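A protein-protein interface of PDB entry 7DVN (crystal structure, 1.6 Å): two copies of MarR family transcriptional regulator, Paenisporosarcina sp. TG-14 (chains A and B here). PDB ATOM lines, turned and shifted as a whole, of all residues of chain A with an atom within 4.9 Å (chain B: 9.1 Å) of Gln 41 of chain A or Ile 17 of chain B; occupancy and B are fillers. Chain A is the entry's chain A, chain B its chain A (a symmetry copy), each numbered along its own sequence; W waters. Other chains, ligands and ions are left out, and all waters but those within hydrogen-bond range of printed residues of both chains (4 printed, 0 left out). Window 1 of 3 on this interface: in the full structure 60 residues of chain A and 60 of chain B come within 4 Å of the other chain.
The backbone carbonyl oxygen of Gly 62 of chain B sits at hydrogen-bond distance from the backbone NH of Glu 38 of chain A, at 3.0 Å.
The side-chain amino group (NZ) of Lys 44 of chain A lies within salt-bridge range of the side-chain carboxylate (OE1) of Glu 13 of chain B, at 3.1 Å.
N of Pro 37 of chain A sits close to O of Gly 62 of chain B.
Of the printed residues of chain B, Pro 37 of chain A touches Gly 62.
Printed residues of chain B within 4 Å of Glu 38 of chain A: Gly 62 (3.0 Å).
Of the printed residues of chain A, Glu 13 of chain B touches Lys 44 (3.1 Å).
Of the printed residues of chain A, Leu 16 of chain B touches Gln 41.
Ile 17 of chain B touches just these residues of chain A: Gln 41 (3.5 Å) and Leu 60 (3.2 Å).
The nearest residue of chain B that does not touch Gln 41 of chain A is Glu 13 of chain B (5.2 Å).
Of the 21 printed residues of chain B, 5 touch a printed residue of chain A.
Hydrophobic or aromatic side chains of chain B within 4 Å of the printed part of chain A: Leu 16 and Ile 17.
Hydrophobic or aromatic side chains of chain A that line the printed part of chain B: Pro 37 and Leu 60.
Among the printed residues, Asp or Glu carboxylates within 4 Å of a Lys or Arg side-chain nitrogen of the other chain: Lys 44 of chain A with Glu 13 of chain B.
3 positions are printed for both chains.
Of the 7 pairs that touch across the chains among the printed residues, none has its exchanged pair printed and touching as well.
Water W3 lies within hydrogen-bond range of the side-chain carboxylate of Glu 13 of chain B and the side-chain amino group of Lys 44 of chain A.
Water W4 bridges the side-chain amide nitrogen (NE2) of Gln 41 of chain A (2.9 Å) and the backbone carbonyl oxygen (O) of Glu 13 of chain B (3.0 Å).
Water W1 bridges O of Gln 61 of chain A (3.0 Å) and N of Glu 38 of chain B (3.3 Å).
Water W2 bridges O of Gln 61 of chain B and N of Glu 38 of chain A.
Among the printed residues, merely in contact across the chains: Leu 60 of chain A with Ile 17 of chain B, Gln 41 of chain A with Ile 17 of chain B, Leu 60 of chain A with Glu 21 of chain B and Gln 41 of chain A with Leu 16 of chain B.
O of Glu 38 of chain A is in hydrogen-bond range of NE2 of Gln 61 of chain A.
The side-chain amide oxygen (OE1) of Gln 41 of chain A is in hydrogen-bond range of the side-chain amide nitrogen (NE2) of Gln 61 of chain A (2.9 Å).
The backbone carbonyl oxygen (O) of Leu 16 of chain B sits at hydrogen-bond distance from the side-chain hydroxyl (OG1) of Thr 20 of chain B, 2.7 Å away.
NH2 of Arg 25 of chain B is in salt-bridge range of OE2 of Glu 21 of chain B, at 2.8 Å.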
ATOM      1  N   PRO A  37     -15.988  22.536 -18.458  1.00  0.00           N
ATOM      2  CA  PRO A  37     -17.216  23.094 -19.030  1.00  0.00           C
ATOM      3  C   PRO A  37     -18.431  22.188 -19.183  1.00  0.00           C
ATOM      4  O   PRO A  37     -19.548  22.552 -19.024  1.00  0.00           O
ATOM      5  CB  PRO A  37     -16.739  23.547 -20.413  1.00  0.00           C
ATOM      6  CG  PRO A  37     -15.319  23.826 -20.220  1.00  0.00           C
ATOM      7  CD  PRO A  37     -14.792  22.786 -19.248  1.00  0.00           C
ATOM      8  N   GLU A  38     -18.211  20.892 -19.475  1.00  0.00           N
ATOM      9  CA  GLU A  38     -19.339  19.954 -19.571  1.00  0.00           C
ATOM     10  C   GLU A  38     -20.057  19.769 -18.207  1.00  0.00           C
ATOM     11  O   GLU A  38     -21.257  19.667 -18.187  1.00  0.00           O
ATOM     12  CB  GLU A  38     -18.825  18.664 -20.225  1.00  0.00           C
ATOM     13  CG  GLU A  38     -17.950  17.801 -19.389  1.00  0.00           C
ATOM     14  CD  GLU A  38     -17.911  16.380 -19.945  1.00  0.00           C
ATOM     15  OE1 GLU A  38     -17.459  15.475 -19.215  1.00  0.00           O
ATOM     16  OE2 GLU A  38     -18.356  16.189 -21.123  1.00  0.00           O
ATOM     17  N   GLN A  39     -19.309  19.801 -17.099  1.00  0.00           N
ATOM     18  CA  GLN A  39     -19.898  19.721 -15.748  1.00  0.00           C
ATOM     19  C   GLN A  39     -20.659  21.018 -15.451  1.00  0.00           C
ATOM     20  O   GLN A  39     -21.780  20.961 -14.960  1.00  0.00           O
ATOM     21  CB  GLN A  39     -18.764  19.510 -14.773  1.00  0.00           C
ATOM     22  CG  GLN A  39     -18.221  18.111 -14.807  1.00  0.00           C
ATOM     23  CD  GLN A  39     -17.022  17.858 -13.936  1.00  0.00           C
ATOM     24  OE1 GLN A  39     -16.181  18.729 -13.666  1.00  0.00           O
ATOM     25  NE2 GLN A  39     -16.939  16.617 -13.448  1.00  0.00           N
ATOM     26  N   MET A  40     -20.056  22.119 -15.825  1.00  0.00           N
ATOM     27  CA  MET A  40     -20.702  23.427 -15.603  1.00  0.00           C
ATOM     28  C   MET A  40     -22.032  23.443 -16.363  1.00  0.00           C
ATOM     29  O   MET A  40     -23.012  23.978 -15.847  1.00  0.00           O
ATOM     30  CB  MET A  40     -19.779  24.560 -16.022  1.00  0.00           C
ATOM     31  CG  MET A  40     -18.514  24.685 -15.195  1.00  0.00           C
ATOM     32  SD  MET A  40     -17.391  25.958 -15.842  1.00  0.00           S
ATOM     33  CE  MET A  40     -16.132  26.110 -14.535  1.00  0.00           C
ATOM     34  N   GLN A  41     -22.114  22.850 -17.564  1.00  0.00           N
ATOM     35  CA  GLN A  41     -23.405  22.782 -18.324  1.00  0.00           C
ATOM     36  C   GLN A  41     -24.498  21.995 -17.592  1.00  0.00           C
ATOM     37  O   GLN A  41     -25.675  22.443 -17.631  1.00  0.00           O
ATOM     38  CB  GLN A  41     -23.129  22.220 -19.721  1.00  0.00           C
ATOM     39  CG  GLN A  41     -24.305  22.340 -20.670  1.00  0.00           C
ATOM     40  CD  GLN A  41     -24.037  21.611 -21.968  1.00  0.00           C
ATOM     41  OE1 GLN A  41     -23.653  20.446 -21.936  1.00  0.00           O
ATOM     42  NE2 GLN A  41     -24.147  22.279 -23.128  1.00  0.00           N
ATOM     43  N   VAL A  42     -24.172  20.896 -16.915  1.00  0.00           N
ATOM     44  CA  VAL A  42     -25.172  20.202 -16.057  1.00  0.00           C
ATOM     45  C   VAL A  42     -25.653  21.177 -14.994  1.00  0.00           C
ATOM     46  O   VAL A  42     -26.840  21.350 -14.868  1.00  0.00           O
ATOM     47  CB  VAL A  42     -24.642  18.921 -15.407  1.00  0.00           C
ATOM     48  CG1 VAL A  42     -25.754  18.216 -14.652  1.00  0.00           C
ATOM     49  CG2 VAL A  42     -23.996  18.014 -16.440  1.00  0.00           C
ATOM     50  N   LEU A  43     -24.740  21.858 -14.302  1.00  0.00           N
ATOM     51  CA  LEU A  43     -25.177  22.747 -13.202  1.00  0.00           C
ATOM     52  C   LEU A  43     -26.042  23.885 -13.750  1.00  0.00           C
ATOM     53  O   LEU A  43     -27.120  24.147 -13.168  1.00  0.00           O
ATOM     54  CB  LEU A  43     -23.953  23.288 -12.467  1.00  0.00           C
ATOM     55  CG  LEU A  43     -22.956  22.254 -11.923  1.00  0.00           C
ATOM     56  CD1 LEU A  43     -21.868  22.977 -11.136  1.00  0.00           C
ATOM     57  CD2 LEU A  43     -23.641  21.231 -11.044  1.00  0.00           C
ATOM     58  N   LYS A  44     -25.639  24.481 -14.892  1.00  0.00           N
ATOM     59  CA  LYS A  44     -26.432  25.632 -15.423  1.00  0.00           C
ATOM     60  C   LYS A  44     -27.802  25.156 -15.938  1.00  0.00           C
ATOM     61  O   LYS A  44     -28.784  25.902 -15.801  1.00  0.00           O
ATOM     62  CB  LYS A  44     -25.632  26.400 -16.479  1.00  0.00           C
ATOM     63  CG  LYS A  44     -26.018  27.853 -16.690  1.00  0.00           C
ATOM     64  CD  LYS A  44     -24.883  28.756 -17.192  1.00  0.00           C
ATOM     65  CE  LYS A  44     -23.817  28.127 -18.079  1.00  0.00           C
ATOM     66  NZ  LYS A  44     -22.509  28.838 -18.103  1.00  0.00           N
ATOM     67  N   LEU A  45     -27.921  23.973 -16.542  1.00  0.00           N
ATOM     68  CA  LEU A  45     -29.221  23.387 -16.944  1.00  0.00           C
ATOM     69  C   LEU A  45     -30.146  23.197 -15.732  1.00  0.00           C
ATOM     70  O   LEU A  45     -31.291  23.642 -15.804  1.00  0.00           O
ATOM     71  CB  LEU A  45     -29.013  22.049 -17.667  1.00  0.00           C
ATOM     72  CG  LEU A  45     -28.816  22.175 -19.174  1.00  0.00           C
ATOM     73  CD1 LEU A  45     -28.422  20.838 -19.760  1.00  0.00           C
ATOM     74  CD2 LEU A  45     -30.077  22.717 -19.830  1.00  0.00           C
ATOM     75  N   LEU A  60     -30.191  17.256 -23.954  1.00  0.00           N
ATOM     76  CA  LEU A  60     -29.790  18.676 -24.013  1.00  0.00           C
ATOM     77  C   LEU A  60     -28.263  18.818 -24.120  1.00  0.00           C
ATOM     78  O   LEU A  60     -27.778  19.765 -24.732  1.00  0.00           O
ATOM     79  CB  LEU A  60     -30.306  19.367 -22.750  1.00  0.00           C
ATOM     80  CG  LEU A  60     -31.818  19.511 -22.688  1.00  0.00           C
ATOM     81  CD1 LEU A  60     -32.302  19.850 -21.283  1.00  0.00           C
ATOM     82  CD2 LEU A  60     -32.316  20.542 -23.683  1.00  0.00           C
ATOM     83  N   GLN A  61     -27.504  17.876 -23.554  1.00  0.00           N
ATOM     84  CA  GLN A  61     -26.036  17.900 -23.637  1.00  0.00           C
ATOM     85  C   GLN A  61     -25.469  17.160 -24.857  1.00  0.00           C
ATOM     86  O   GLN A  61     -24.253  17.234 -25.030  1.00  0.00           O
ATOM     87  CB  GLN A  61     -25.447  17.215 -22.408  1.00  0.00           C
ATOM     88  CG  GLN A  61     -25.693  17.974 -21.134  1.00  0.00           C
ATOM     89  CD  GLN A  61     -24.705  17.559 -20.079  1.00  0.00           C
ATOM     90  OE1 GLN A  61     -24.799  16.460 -19.515  1.00  0.00           O
ATOM     91  NE2 GLN A  61     -23.705  18.404 -19.866  1.00  0.00           N
ATOM     92  N   VAL B   9     -23.380  35.506 -23.884  1.00  0.00           N
ATOM     93  CA  VAL B   9     -22.750  34.172 -23.644  1.00  0.00           C
ATOM     94  C   VAL B   9     -23.842  33.181 -23.250  1.00  0.00           C
ATOM     95  O   VAL B   9     -23.822  32.054 -23.771  1.00  0.00           O
ATOM     96  CB  VAL B   9     -21.635  34.310 -22.591  1.00  0.00           C
ATOM     97  CG1 VAL B   9     -21.110  32.939 -22.151  1.00  0.00           C
ATOM     98  CG2 VAL B   9     -20.493  35.162 -23.068  1.00  0.00           C
ATOM     99  N   SER B  10     -24.763  33.561 -22.368  1.00  0.00           N
ATOM    100  CA  SER B  10     -25.892  32.688 -21.941  1.00  0.00           C
ATOM    101  C   SER B  10     -26.730  32.293 -23.173  1.00  0.00           C
ATOM    102  O   SER B  10     -27.053  31.112 -23.347  1.00  0.00           O
ATOM    103  CB  SER B  10     -26.733  33.389 -20.926  1.00  0.00           C
ATOM    104  OG  SER B  10     -26.863  34.784 -21.268  1.00  0.00           O
ATOM    105  N   LEU B  11     -27.015  33.253 -24.046  1.00  0.00           N
ATOM    106  CA  LEU B  11     -27.821  32.942 -25.249  1.00  0.00           C
ATOM    107  C   LEU B  11     -27.106  31.951 -26.143  1.00  0.00           C
ATOM    108  O   LEU B  11     -27.731  31.078 -26.770  1.00  0.00           O
ATOM    109  CB  LEU B  11     -28.170  34.221 -26.012  1.00  0.00           C
ATOM    110  CG  LEU B  11     -29.316  35.042 -25.436  1.00  0.00           C
ATOM    111  CD1 LEU B  11     -29.370  36.439 -26.099  1.00  0.00           C
ATOM    112  CD2 LEU B  11     -30.638  34.347 -25.584  1.00  0.00           C
ATOM    113  N   PHE B  12     -25.795  32.121 -26.336  1.00  0.00           N
ATOM    114  CA  PHE B  12     -24.951  31.234 -27.147  1.00  0.00           C
ATOM    115  C   PHE B  12     -25.100  29.813 -26.594  1.00  0.00           C
ATOM    116  O   PHE B  12     -25.339  28.888 -27.339  1.00  0.00           O
ATOM    117  CB  PHE B  12     -23.510  31.734 -27.131  1.00  0.00           C
ATOM    118  CG  PHE B  12     -22.624  30.854 -27.944  1.00  0.00           C
ATOM    119  CD1 PHE B  12     -22.519  31.001 -29.320  1.00  0.00           C
ATOM    120  CD2 PHE B  12     -21.939  29.789 -27.371  1.00  0.00           C
ATOM    121  CE1 PHE B  12     -21.728  30.172 -30.079  1.00  0.00           C
ATOM    122  CE2 PHE B  12     -21.126  28.966 -28.157  1.00  0.00           C
ATOM    123  CZ  PHE B  12     -21.074  29.128 -29.518  1.00  0.00           C
ATOM    124  N   GLU B  13     -24.967  29.668 -25.282  1.00  0.00           N
ATOM    125  CA  GLU B  13     -25.023  28.342 -24.613  1.00  0.00           C
ATOM    126  C   GLU B  13     -26.428  27.746 -24.769  1.00  0.00           C
ATOM    127  O   GLU B  13     -26.524  26.538 -24.949  1.00  0.00           O
ATOM    128  CB  GLU B  13     -24.658  28.498 -23.151  1.00  0.00           C
ATOM    129  CG  GLU B  13     -23.197  28.838 -22.913  1.00  0.00           C
ATOM    130  CD  GLU B  13     -22.847  29.245 -21.487  1.00  0.00           C
ATOM    131  OE1 GLU B  13     -23.739  29.642 -20.777  1.00  0.00           O
ATOM    132  OE2 GLU B  13     -21.639  29.114 -21.142  1.00  0.00           O
ATOM    133  N   GLU B  14     -27.453  28.546 -24.698  1.00  0.00           N
ATOM    134  CA  GLU B  14     -28.863  28.096 -24.867  1.00  0.00           C
ATOM    135  C   GLU B  14     -29.100  27.674 -26.297  1.00  0.00           C
ATOM    136  O   GLU B  14     -29.825  26.686 -26.553  1.00  0.00           O
ATOM    137  CB  GLU B  14     -29.792  29.196 -24.428  1.00  0.00           C
ATOM    138  CG  GLU B  14     -29.773  29.312 -22.905  1.00  0.00           C
ATOM    139  CD  GLU B  14     -30.265  30.597 -22.308  1.00  0.00           C
ATOM    140  OE1 GLU B  14     -30.872  31.415 -23.000  1.00  0.00           O
ATOM    141  OE2 GLU B  14     -29.933  30.802 -21.114  1.00  0.00           O
ATOM    142  N   VAL B  15     -28.629  28.440 -27.274  1.00  0.00           N
ATOM    143  CA  VAL B  15     -28.803  28.009 -28.677  1.00  0.00           C
ATOM    144  C   VAL B  15     -28.127  26.660 -28.905  1.00  0.00           C
ATOM    145  O   VAL B  15     -28.736  25.786 -29.558  1.00  0.00           O
ATOM    146  CB  VAL B  15     -28.308  29.112 -29.633  1.00  0.00           C
ATOM    147  CG1 VAL B  15     -28.014  28.588 -31.024  1.00  0.00           C
ATOM    148  CG2 VAL B  15     -29.324  30.234 -29.649  1.00  0.00           C
ATOM    149  N   LEU B  16     -26.971  26.406 -28.284  1.00  0.00           N
ATOM    150  CA  LEU B  16     -26.332  25.086 -28.382  1.00  0.00           C
ATOM    151  C   LEU B  16     -27.271  23.995 -27.793  1.00  0.00           C
ATOM    152  O   LEU B  16     -27.518  22.981 -28.494  1.00  0.00           O
ATOM    153  CB  LEU B  16     -25.002  25.130 -27.628  1.00  0.00           C
ATOM    154  CG  LEU B  16     -24.325  23.761 -27.510  1.00  0.00           C
ATOM    155  CD1 LEU B  16     -23.964  23.202 -28.853  1.00  0.00           C
ATOM    156  CD2 LEU B  16     -23.139  23.884 -26.551  1.00  0.00           C
ATOM    157  N   ILE B  17     -27.761  24.190 -26.585  1.00  0.00           N
ATOM    158  CA  ILE B  17     -28.556  23.118 -25.912  1.00  0.00           C
ATOM    159  C   ILE B  17     -29.859  22.906 -26.648  1.00  0.00           C
ATOM    160  O   ILE B  17     -30.189  21.749 -27.004  1.00  0.00           O
ATOM    161  CB  ILE B  17     -28.799  23.487 -24.459  1.00  0.00           C
ATOM    162  CG1 ILE B  17     -27.477  23.281 -23.720  1.00  0.00           C
ATOM    163  CG2 ILE B  17     -29.967  22.718 -23.853  1.00  0.00           C
ATOM    164  CD1 ILE B  17     -27.327  24.193 -22.537  1.00  0.00           C
ATOM    165  N   TYR B  18     -30.556  23.998 -26.932  1.00  0.00           N
ATOM    166  CA  TYR B  18     -31.901  23.845 -27.543  1.00  0.00           C
ATOM    167  C   TYR B  18     -31.802  23.405 -28.985  1.00  0.00           C
ATOM    168  O   TYR B  18     -32.685  22.676 -29.479  1.00  0.00           O
ATOM    169  CB  TYR B  18     -32.755  25.096 -27.356  1.00  0.00           C
ATOM    170  CG  TYR B  18     -33.082  25.241 -25.892  1.00  0.00           C
ATOM    171  CD1 TYR B  18     -33.670  24.198 -25.192  1.00  0.00           C
ATOM    172  CD2 TYR B  18     -32.579  26.312 -25.182  1.00  0.00           C
ATOM    173  CE1 TYR B  18     -33.848  24.269 -23.816  1.00  0.00           C
ATOM    174  CE2 TYR B  18     -32.763  26.407 -23.816  1.00  0.00           C
ATOM    175  CZ  TYR B  18     -33.384  25.380 -23.132  1.00  0.00           C
ATOM    176  OH  TYR B  18     -33.541  25.489 -21.778  1.00  0.00           O
ATOM    177  N   GLY B  19     -30.799  23.872 -29.741  1.00  0.00           N
ATOM    178  CA  GLY B  19     -30.572  23.364 -31.083  1.00  0.00           C
ATOM    179  C   GLY B  19     -30.219  21.876 -31.070  1.00  0.00           C
ATOM    180  O   GLY B  19     -30.675  21.174 -31.961  1.00  0.00           O
ATOM    181  N   THR B  20     -29.360  21.441 -30.141  1.00  0.00           N
ATOM    182  CA  THR B  20     -28.973  20.029 -29.978  1.00  0.00           C
ATOM    183  C   THR B  20     -30.245  19.201 -29.763  1.00  0.00           C
ATOM    184  O   THR B  20     -30.443  18.254 -30.513  1.00  0.00           O
ATOM    185  CB  THR B  20     -27.966  19.847 -28.871  1.00  0.00           C
ATOM    186  OG1 THR B  20     -26.752  20.507 -29.205  1.00  0.00           O
ATOM    187  CG2 THR B  20     -27.642  18.378 -28.690  1.00  0.00           C
ATOM    188  N   GLU B  21     -31.092  19.614 -28.839  1.00  0.00           N
ATOM    189  CA  GLU B  21     -32.343  18.875 -28.537  1.00  0.00           C
ATOM    190  C   GLU B  21     -33.218  18.847 -29.777  1.00  0.00           C
ATOM    191  O   GLU B  21     -33.765  17.787 -30.122  1.00  0.00           O
ATOM    192  CB  GLU B  21     -33.051  19.538 -27.366  1.00  0.00           C
ATOM    193  CG  GLU B  21     -34.437  19.004 -27.144  1.00  0.00           C
ATOM    194  CD  GLU B  21     -35.238  19.655 -26.058  1.00  0.00           C
ATOM    195  OE1 GLU B  21     -35.208  20.880 -25.884  1.00  0.00           O
ATOM    196  OE2 GLU B  21     -36.033  18.885 -25.425  1.00  0.00           O
ATOM    197  N   ARG B  22     -33.390  19.997 -30.433  1.00  0.00           N
ATOM    198  CA  ARG B  22     -34.255  20.063 -31.635  1.00  0.00           C
ATOM    199  C   ARG B  22     -33.788  19.037 -32.658  1.00  0.00           C
ATOM    200  O   ARG B  22     -34.618  18.309 -33.248  1.00  0.00           O
ATOM    201  CB  ARG B  22     -34.230  21.468 -32.215  1.00  0.00           C
ATOM    202  CG  ARG B  22     -34.961  21.608 -33.526  1.00  0.00           C
ATOM    203  CD  ARG B  22     -36.466  21.597 -33.343  1.00  0.00           C
ATOM    204  NE  ARG B  22     -37.012  22.850 -32.806  1.00  0.00           N
ATOM    205  CZ  ARG B  22     -38.304  23.193 -32.853  1.00  0.00           C
ATOM    206  NH1 ARG B  22     -38.714  24.322 -32.313  1.00  0.00           N
ATOM    207  NH2 ARG B  22     -39.190  22.370 -33.364  1.00  0.00           N
ATOM    208  N   VAL B  23     -32.481  19.000 -32.942  1.00  0.00           N
ATOM    209  CA  VAL B  23     -31.995  18.113 -34.010  1.00  0.00           C
ATOM    210  C   VAL B  23     -32.184  16.663 -33.564  1.00  0.00           C
ATOM    211  O   VAL B  23     -32.759  15.911 -34.357  1.00  0.00           O
ATOM    212  CB  VAL B  23     -30.545  18.446 -34.341  1.00  0.00           C
ATOM    213  CG1 VAL B  23     -30.024  17.418 -35.310  1.00  0.00           C
ATOM    214  CG2 VAL B  23     -30.415  19.849 -34.886  1.00  0.00           C
ATOM    215  N   ILE B  24     -31.758  16.292 -32.364  1.00  0.00           N
ATOM    216  CA  ILE B  24     -31.830  14.870 -31.901  1.00  0.00           C
ATOM    217  C   ILE B  24     -33.289  14.412 -31.976  1.00  0.00           C
ATOM    218  O   ILE B  24     -33.574  13.317 -32.507  1.00  0.00           O
ATOM    219  CB  ILE B  24     -31.242  14.710 -30.492  1.00  0.00           C
ATOM    220  CG1 ILE B  24     -29.725  14.876 -30.457  1.00  0.00           C
ATOM    221  CG2 ILE B  24     -31.662  13.371 -29.878  1.00  0.00           C
ATOM    222  CD1 ILE B  24     -29.127  14.907 -29.055  1.00  0.00           C
ATOM    223  N   ARG B  25     -34.211  15.265 -31.569  1.00  0.00           N
ATOM    224  CA  ARG B  25     -35.653  14.899 -31.507  1.00  0.00           C
ATOM    225  C   ARG B  25     -36.322  14.944 -32.878  1.00  0.00           C
ATOM    226  O   ARG B  25     -37.410  14.374 -32.961  1.00  0.00           O
ATOM    227  CB  ARG B  25     -36.383  15.764 -30.470  1.00  0.00           C
ATOM    228  CG  ARG B  25     -35.944  15.506 -29.033  1.00  0.00           C
ATOM    229  CD  ARG B  25     -36.648  16.301 -27.940  1.00  0.00           C
ATOM    230  NE  ARG B  25     -38.100  16.233 -27.995  1.00  0.00           N
ATOM    231  CZ  ARG B  25     -38.917  17.032 -27.301  1.00  0.00           C
ATOM    232  NH1 ARG B  25     -40.227  16.898 -27.411  1.00  0.00           N
ATOM    233  NH2 ARG B  25     -38.426  17.948 -26.483  1.00  0.00           N
ATOM    234  N   PRO B  37     -24.216  13.682 -30.471  1.00  0.00           N
ATOM    235  CA  PRO B  37     -23.440  14.859 -30.870  1.00  0.00           C
ATOM    236  C   PRO B  37     -22.035  15.035 -30.308  1.00  0.00           C
ATOM    237  O   PRO B  37     -21.132  15.490 -30.925  1.00  0.00           O
ATOM    238  CB  PRO B  37     -24.332  16.003 -30.378  1.00  0.00           C
ATOM    239  CG  PRO B  37     -25.678  15.436 -30.410  1.00  0.00           C
ATOM    240  CD  PRO B  37     -25.556  13.982 -29.989  1.00  0.00           C
ATOM    241  N   GLU B  38     -21.806  14.606 -29.052  1.00  0.00           N
ATOM    242  CA  GLU B  38     -20.455  14.688 -28.478  1.00  0.00           C
ATOM    243  C   GLU B  38     -19.451  13.771 -29.226  1.00  0.00           C
ATOM    244  O   GLU B  38     -18.325  14.161 -29.407  1.00  0.00           O
ATOM    245  CB  GLU B  38     -20.569  14.444 -26.967  1.00  0.00           C
ATOM    246  CG  GLU B  38     -20.857  13.049 -26.541  1.00  0.00           C
ATOM    247  CD  GLU B  38     -20.473  12.845 -25.078  1.00  0.00           C
ATOM    248  OE1 GLU B  38     -20.385  11.677 -24.650  1.00  0.00           O
ATOM    249  OE2 GLU B  38     -20.248  13.882 -24.372  1.00  0.00           O
ATOM    250  N   GLN B  61     -13.148  20.060 -26.335  1.00  0.00           N
ATOM    251  CA  GLN B  61     -14.498  19.583 -25.999  1.00  0.00           C
ATOM    252  C   GLN B  61     -14.987  20.025 -24.612  1.00  0.00           C
ATOM    253  O   GLN B  61     -16.148  19.740 -24.322  1.00  0.00           O
ATOM    254  CB  GLN B  61     -14.511  18.058 -25.993  1.00  0.00           C
ATOM    255  CG  GLN B  61     -14.308  17.460 -27.357  1.00  0.00           C
ATOM    256  CD  GLN B  61     -14.819  16.047 -27.391  1.00  0.00           C
ATOM    257  OE1 GLN B  61     -14.201  15.132 -26.830  1.00  0.00           O
ATOM    258  NE2 GLN B  61     -15.995  15.877 -27.982  1.00  0.00           N
ATOM    259  N   GLY B  62     -14.125  20.639 -23.819  1.00  0.00           N
ATOM    260  CA  GLY B  62     -14.469  21.084 -22.460  1.00  0.00           C
ATOM    261  C   GLY B  62     -14.690  19.906 -21.531  1.00  0.00           C
ATOM    262  O   GLY B  62     -15.680  19.948 -20.772  1.00  0.00           O
HETATM  263  O   HOH W   1     -22.116  17.313 -27.165  1.00  0.00           O
HETATM  264  O   HOH W   2     -18.555  20.698 -22.766  1.00  0.00           O
HETATM  265  O   HOH W   3     -23.328  31.934 -19.345  1.00  0.00           O
HETATM  266  O   HOH W   4     -24.432  25.137 -23.228  1.00  0.00           O
